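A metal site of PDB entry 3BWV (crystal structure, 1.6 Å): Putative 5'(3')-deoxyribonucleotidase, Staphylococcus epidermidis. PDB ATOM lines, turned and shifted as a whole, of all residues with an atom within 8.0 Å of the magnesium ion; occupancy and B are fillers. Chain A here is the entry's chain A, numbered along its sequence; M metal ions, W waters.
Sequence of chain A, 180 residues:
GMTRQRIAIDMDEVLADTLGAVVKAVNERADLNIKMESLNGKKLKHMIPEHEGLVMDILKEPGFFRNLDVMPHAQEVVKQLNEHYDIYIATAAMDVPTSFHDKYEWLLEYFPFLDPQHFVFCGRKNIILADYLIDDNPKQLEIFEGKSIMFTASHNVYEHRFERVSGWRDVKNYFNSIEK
Water W2 bridges OD1 of Asp 10 (2.9 Å) and N of Asp 12 (3.5 Å).
The magnesium ion is bound by water W2 (2.0 Å), OD2 of Asp 10 (2.0 Å), water W1 (2.0 Å), OD1 of Asp 136 (2.1 Å), O of Asp 12 (2.1 Å) and water W3 (2.1 Å).
The magnesium ion has six donor atoms within binding distance.
The side-chain carboxylate of Asp 10 is in salt-bridge range of the side-chain amino group of Lys 125 (2.8 Å).
The backbone carbonyl oxygen of Ile 134 is in hydrogen-bond range of the backbone NH of Asp 10, 3.0 Å away.
A ring nitrogen (NE2) of His 155 is in hydrogen-bond range of the side-chain carboxylate (OD2) of Asp 136, at 2.8 Å.
The side-chain carboxylate (OD1) of Asp 12 sits at hydrogen-bond distance from the side-chain hydroxyl (OG1) of Thr 18 (2.7 Å).
OD2 of Asp 12 lies within salt-bridge range of NZ of Lys 103, at 2.7 Å.
OD1 of Asp 135 is in hydrogen-bond range of N of Asn 137, at 2.9 Å.
The side-chain carboxylate (OD2) of Asp 135 is in salt-bridge range of the side-chain amino group (NZ) of Lys 125 (2.8 Å).
O of Asp 135 sits at hydrogen-bond distance from N of Phe 151 (3.0 Å).
Merely in contact with the magnesium ion: Asp 135.
Within 4 Å of the magnesium ion: Asp 10, Asp 12, Asp 135 and Asp 136.
The nearest printed residue that does not touch the magnesium ion is Glu 13 (4.4 Å).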
ATOM      1  N   ILE A   9      12.686 -16.474  26.492  1.00  0.00           N
ATOM      2  CA  ILE A   9      13.153 -15.215  25.856  1.00  0.00           C
ATOM      3  C   ILE A   9      14.599 -14.927  26.382  1.00  0.00           C
ATOM      4  O   ILE A   9      14.857 -14.920  27.559  1.00  0.00           O
ATOM      5  CB  ILE A   9      12.230 -14.077  26.158  1.00  0.00           C
ATOM      6  CG1 ILE A   9      10.844 -14.524  25.798  1.00  0.00           C
ATOM      7  CG2 ILE A   9      12.645 -12.793  25.395  1.00  0.00           C
ATOM      8  CD1 ILE A   9       9.802 -13.456  26.138  1.00  0.00           C
ATOM      9  N   ASP A  10      15.517 -14.676  25.450  1.00  0.00           N
ATOM     10  CA  ASP A  10      16.884 -14.281  25.722  1.00  0.00           C
ATOM     11  C   ASP A  10      16.915 -12.830  26.166  1.00  0.00           C
ATOM     12  O   ASP A  10      16.066 -12.096  25.779  1.00  0.00           O
ATOM     13  CB  ASP A  10      17.687 -14.447  24.450  1.00  0.00           C
ATOM     14  CG  ASP A  10      19.164 -14.024  24.571  1.00  0.00           C
ATOM     15  OD1 ASP A  10      19.900 -14.562  25.446  1.00  0.00           O
ATOM     16  OD2 ASP A  10      19.565 -13.220  23.666  1.00  0.00           O
ATOM     17  N   MET A  11      17.917 -12.435  26.958  1.00  0.00           N
ATOM     18  CA  MET A  11      18.089 -11.048  27.350  1.00  0.00           C
ATOM     19  C   MET A  11      18.842 -10.174  26.349  1.00  0.00           C
ATOM     20  O   MET A  11      18.270  -9.253  25.745  1.00  0.00           O
ATOM     21  CB  MET A  11      18.760 -10.970  28.722  1.00  0.00           C
ATOM     22  CG  MET A  11      17.856 -11.513  29.804  1.00  0.00           C
ATOM     23  SD  MET A  11      18.459 -11.093  31.591  1.00  0.00           S
ATOM     24  CE  MET A  11      17.719  -9.296  31.771  1.00  0.00           C
ATOM     25  N   ASP A  12      20.110 -10.465  26.116  1.00  0.00           N
ATOM     26  CA  ASP A  12      20.959  -9.491  25.422  1.00  0.00           C
ATOM     27  C   ASP A  12      20.676  -9.482  23.933  1.00  0.00           C
ATOM     28  O   ASP A  12      20.686 -10.524  23.271  1.00  0.00           O
ATOM     29  CB  ASP A  12      22.435  -9.686  25.725  1.00  0.00           C
ATOM     30  CG  ASP A  12      22.763  -9.390  27.177  1.00  0.00           C
ATOM     31  OD1 ASP A  12      22.485  -8.233  27.643  1.00  0.00           O
ATOM     32  OD2 ASP A  12      23.302 -10.286  27.861  1.00  0.00           O
ATOM     33  N   GLU A  13      20.390  -8.277  23.440  1.00  0.00           N
ATOM     34  CA  GLU A  13      20.058  -7.982  22.054  1.00  0.00           C
ATOM     35  C   GLU A  13      18.659  -8.496  21.713  1.00  0.00           C
ATOM     36  O   GLU A  13      18.333  -8.549  20.514  1.00  0.00           O
ATOM     37  CB  GLU A  13      21.138  -8.529  21.100  1.00  0.00           C
ATOM     38  CG  GLU A  13      22.486  -7.897  21.314  1.00  0.00           C
ATOM     39  CD  GLU A  13      23.447  -7.956  20.142  1.00  0.00           C
ATOM     40  OE1 GLU A  13      23.139  -7.421  19.026  1.00  0.00           O
ATOM     41  OE2 GLU A  13      24.567  -8.485  20.336  1.00  0.00           O
ATOM     42  N   VAL A  14      17.796  -8.723  22.730  1.00  0.00           N
ATOM     43  CA  VAL A  14      16.419  -9.208  22.539  1.00  0.00           C
ATOM     44  C   VAL A  14      15.534  -8.425  23.436  1.00  0.00           C
ATOM     45  O   VAL A  14      14.800  -7.551  22.967  1.00  0.00           O
ATOM     46  CB  VAL A  14      16.298 -10.752  22.755  1.00  0.00           C
ATOM     47  CG1 VAL A  14      14.824 -11.200  22.812  1.00  0.00           C
ATOM     48  CG2 VAL A  14      17.121 -11.463  21.704  1.00  0.00           C
ATOM     49  N   LEU A  15      15.645  -8.619  24.764  1.00  0.00           N
ATOM     50  CA  LEU A  15      14.864  -7.781  25.674  1.00  0.00           C
ATOM     51  C   LEU A  15      15.549  -6.453  25.974  1.00  0.00           C
ATOM     52  O   LEU A  15      14.923  -5.430  26.175  1.00  0.00           O
ATOM     53  CB  LEU A  15      14.611  -8.482  27.016  1.00  0.00           C
ATOM     54  CG  LEU A  15      13.630  -9.673  27.014  1.00  0.00           C
ATOM     55  CD1 LEU A  15      13.695 -10.334  28.369  1.00  0.00           C
ATOM     56  CD2 LEU A  15      12.224  -9.123  26.776  1.00  0.00           C
ATOM     57  N   ALA A  16      16.879  -6.488  25.954  1.00  0.00           N
ATOM     58  CA  ALA A  16      17.752  -5.386  26.385  1.00  0.00           C
ATOM     59  C   ALA A  16      18.612  -4.947  25.229  1.00  0.00           C
ATOM     60  O   ALA A  16      19.211  -5.763  24.524  1.00  0.00           O
ATOM     61  CB  ALA A  16      18.631  -5.814  27.543  1.00  0.00           C
ATOM     62  N   THR A  18      21.599  -4.193  24.394  1.00  0.00           N
ATOM     63  CA  THR A  18      22.995  -4.332  24.809  1.00  0.00           C
ATOM     64  C   THR A  18      23.965  -3.702  23.816  1.00  0.00           C
ATOM     65  O   THR A  18      24.975  -3.128  24.192  1.00  0.00           O
ATOM     66  CB  THR A  18      23.380  -5.819  24.969  1.00  0.00           C
ATOM     67  OG1 THR A  18      22.294  -6.516  25.580  1.00  0.00           O
ATOM     68  CG2 THR A  18      24.599  -5.956  25.833  1.00  0.00           C
ATOM     69  N   ALA A  90      15.864 -16.452  29.765  1.00  0.00           N
ATOM     70  CA  ALA A  90      17.060 -17.260  29.762  1.00  0.00           C
ATOM     71  C   ALA A  90      18.289 -16.377  29.457  1.00  0.00           C
ATOM     72  O   ALA A  90      18.250 -15.513  28.586  1.00  0.00           O
ATOM     73  CB  ALA A  90      16.900 -18.363  28.767  1.00  0.00           C
ATOM     74  N   THR A  91      19.357 -16.514  30.215  1.00  0.00           N
ATOM     75  CA  THR A  91      20.548 -15.688  29.962  1.00  0.00           C
ATOM     76  C   THR A  91      21.766 -16.410  30.513  1.00  0.00           C
ATOM     77  O   THR A  91      21.620 -17.252  31.383  1.00  0.00           O
ATOM     78  CB  THR A  91      20.346 -14.234  30.593  1.00  0.00           C
ATOM     79  OG1 THR A  91      21.445 -13.355  30.224  1.00  0.00           O
ATOM     80  CG2 THR A  91      20.146 -14.269  32.172  1.00  0.00           C
ATOM     81  N   LYS A 103      21.459  -8.180  36.099  1.00  0.00           N
ATOM     82  CA  LYS A 103      20.426  -8.713  35.224  1.00  0.00           C
ATOM     83  C   LYS A 103      19.123  -8.972  35.968  1.00  0.00           C
ATOM     84  O   LYS A 103      18.057  -8.657  35.466  1.00  0.00           O
ATOM     85  CB  LYS A 103      20.932  -9.948  34.555  1.00  0.00           C
ATOM     86  CG  LYS A 103      21.899  -9.659  33.449  1.00  0.00           C
ATOM     87  CD  LYS A 103      22.550 -10.911  32.892  1.00  0.00           C
ATOM     88  CE  LYS A 103      23.276 -10.653  31.605  1.00  0.00           C
ATOM     89  NZ  LYS A 103      22.402 -10.527  30.409  1.00  0.00           N
ATOM     90  N   LYS A 125      21.181 -23.288  25.693  1.00  0.00           N
ATOM     91  CA  LYS A 125      19.756 -23.304  25.875  1.00  0.00           C
ATOM     92  C   LYS A 125      19.059 -24.579  25.354  1.00  0.00           C
ATOM     93  O   LYS A 125      17.831 -24.622  25.418  1.00  0.00           O
ATOM     94  CB  LYS A 125      19.173 -22.061  25.217  1.00  0.00           C
ATOM     95  CG  LYS A 125      19.551 -20.714  25.894  1.00  0.00           C
ATOM     96  CD  LYS A 125      18.917 -19.571  25.182  1.00  0.00           C
ATOM     97  CE  LYS A 125      19.048 -18.159  25.852  1.00  0.00           C
ATOM     98  NZ  LYS A 125      20.198 -17.316  25.376  1.00  0.00           N
ATOM     99  N   ILE A 134      12.793 -17.187  21.791  1.00  0.00           N
ATOM    100  CA  ILE A 134      13.126 -15.992  21.054  1.00  0.00           C
ATOM    101  C   ILE A 134      14.557 -15.606  21.440  1.00  0.00           C
ATOM    102  O   ILE A 134      14.842 -15.243  22.573  1.00  0.00           O
ATOM    103  CB  ILE A 134      12.156 -14.856  21.369  1.00  0.00           C
ATOM    104  CG1 ILE A 134      10.704 -15.300  21.189  1.00  0.00           C
ATOM    105  CG2 ILE A 134      12.454 -13.566  20.516  1.00  0.00           C
ATOM    106  CD1 ILE A 134       9.689 -14.303  21.681  1.00  0.00           C
ATOM    107  N   ASP A 135      15.462 -15.665  20.480  1.00  0.00           N
ATOM    108  CA  ASP A 135      16.914 -15.453  20.731  1.00  0.00           C
ATOM    109  C   ASP A 135      17.548 -14.818  19.501  1.00  0.00           C
ATOM    110  O   ASP A 135      17.108 -15.114  18.357  1.00  0.00           O
ATOM    111  CB  ASP A 135      17.593 -16.813  21.052  1.00  0.00           C
ATOM    112  CG  ASP A 135      18.901 -16.704  21.789  1.00  0.00           C
ATOM    113  OD1 ASP A 135      19.758 -15.880  21.401  1.00  0.00           O
ATOM    114  OD2 ASP A 135      19.139 -17.498  22.763  1.00  0.00           O
ATOM    115  N   ASP A 136      18.576 -14.016  19.678  1.00  0.00           N
ATOM    116  CA  ASP A 136      19.350 -13.534  18.524  1.00  0.00           C
ATOM    117  C   ASP A 136      20.516 -14.423  18.025  1.00  0.00           C
ATOM    118  O   ASP A 136      21.059 -14.209  16.946  1.00  0.00           O
ATOM    119  CB  ASP A 136      19.821 -12.094  18.838  1.00  0.00           C
ATOM    120  CG  ASP A 136      20.826 -12.075  19.966  1.00  0.00           C
ATOM    121  OD1 ASP A 136      20.501 -12.534  21.054  1.00  0.00           O
ATOM    122  OD2 ASP A 136      21.992 -11.663  19.711  1.00  0.00           O
ATOM    123  N   ASN A 137      20.922 -15.412  18.810  1.00  0.00           N
ATOM    124  CA  ASN A 137      22.114 -16.160  18.531  1.00  0.00           C
ATOM    125  C   ASN A 137      21.773 -17.455  17.789  1.00  0.00           C
ATOM    126  O   ASN A 137      21.122 -18.327  18.358  1.00  0.00           O
ATOM    127  CB  ASN A 137      22.791 -16.459  19.842  1.00  0.00           C
ATOM    128  CG  ASN A 137      24.099 -17.186  19.658  1.00  0.00           C
ATOM    129  OD1 ASN A 137      24.554 -17.450  18.532  1.00  0.00           O
ATOM    130  ND2 ASN A 137      24.756 -17.507  20.770  1.00  0.00           N
ATOM    131  N   GLN A 140      22.415 -20.880  19.548  1.00  0.00           N
ATOM    132  CA  GLN A 140      21.407 -21.261  20.544  1.00  0.00           C
ATOM    133  C   GLN A 140      20.159 -21.779  19.823  1.00  0.00           C
ATOM    134  O   GLN A 140      19.607 -22.850  20.187  1.00  0.00           O
ATOM    135  CB  GLN A 140      21.029 -20.057  21.438  1.00  0.00           C
ATOM    136  CG  GLN A 140      22.111 -19.518  22.365  1.00  0.00           C
ATOM    137  CD  GLN A 140      22.584 -20.474  23.475  1.00  0.00           C
ATOM    138  OE1 GLN A 140      22.285 -21.674  23.483  1.00  0.00           O
ATOM    139  NE2 GLN A 140      23.414 -19.936  24.370  1.00  0.00           N
ATOM    140  N   PHE A 151      15.364 -13.376  16.624  1.00  0.00           N
ATOM    141  CA  PHE A 151      15.154 -11.957  16.796  1.00  0.00           C
ATOM    142  C   PHE A 151      16.291 -11.197  16.094  1.00  0.00           C
ATOM    143  O   PHE A 151      17.469 -11.459  16.319  1.00  0.00           O
ATOM    144  CB  PHE A 151      15.170 -11.634  18.261  1.00  0.00           C
ATOM    145  CG  PHE A 151      14.651 -10.266  18.593  1.00  0.00           C
ATOM    146  CD1 PHE A 151      13.300  -9.986  18.849  1.00  0.00           C
ATOM    147  CD2 PHE A 151      15.541  -9.197  18.649  1.00  0.00           C
ATOM    148  CE1 PHE A 151      12.868  -8.688  19.175  1.00  0.00           C
ATOM    149  CE2 PHE A 151      15.096  -7.925  19.000  1.00  0.00           C
ATOM    150  CZ  PHE A 151      13.758  -7.670  19.236  1.00  0.00           C
ATOM    151  N   ALA A 153      19.217  -9.010  14.821  1.00  0.00           N
ATOM    152  CA  ALA A 153      20.308  -8.244  15.352  1.00  0.00           C
ATOM    153  C   ALA A 153      21.332  -8.033  14.241  1.00  0.00           C
ATOM    154  O   ALA A 153      21.404  -8.823  13.305  1.00  0.00           O
ATOM    155  CB  ALA A 153      20.971  -8.972  16.515  1.00  0.00           C
ATOM    156  N   HIS A 155      24.434  -8.687  13.930  1.00  0.00           N
ATOM    157  CA  HIS A 155      25.309  -9.816  13.669  1.00  0.00           C
ATOM    158  C   HIS A 155      24.643 -10.967  12.869  1.00  0.00           C
ATOM    159  O   HIS A 155      25.348 -11.751  12.240  1.00  0.00           O
ATOM    160  CB  HIS A 155      25.919 -10.291  15.018  1.00  0.00           C
ATOM    161  CG  HIS A 155      24.965 -11.054  15.889  1.00  0.00           C
ATOM    162  ND1 HIS A 155      24.749 -12.384  15.701  1.00  0.00           N
ATOM    163  CD2 HIS A 155      24.147 -10.668  16.911  1.00  0.00           C
ATOM    164  CE1 HIS A 155      23.844 -12.811  16.568  1.00  0.00           C
ATOM    165  NE2 HIS A 155      23.449 -11.784  17.296  1.00  0.00           N
HETATM  166 MG    MG M   1      21.280 -12.538  22.960  1.00  0.00          MG
HETATM  167  O   HOH W   1      21.814 -14.389  22.458  1.00  0.00           O
HETATM  168  O   HOH W   2      22.150 -12.876  24.699  1.00  0.00           O
HETATM  169  O   HOH W   3      23.075 -11.727  22.143  1.00  0.00           O
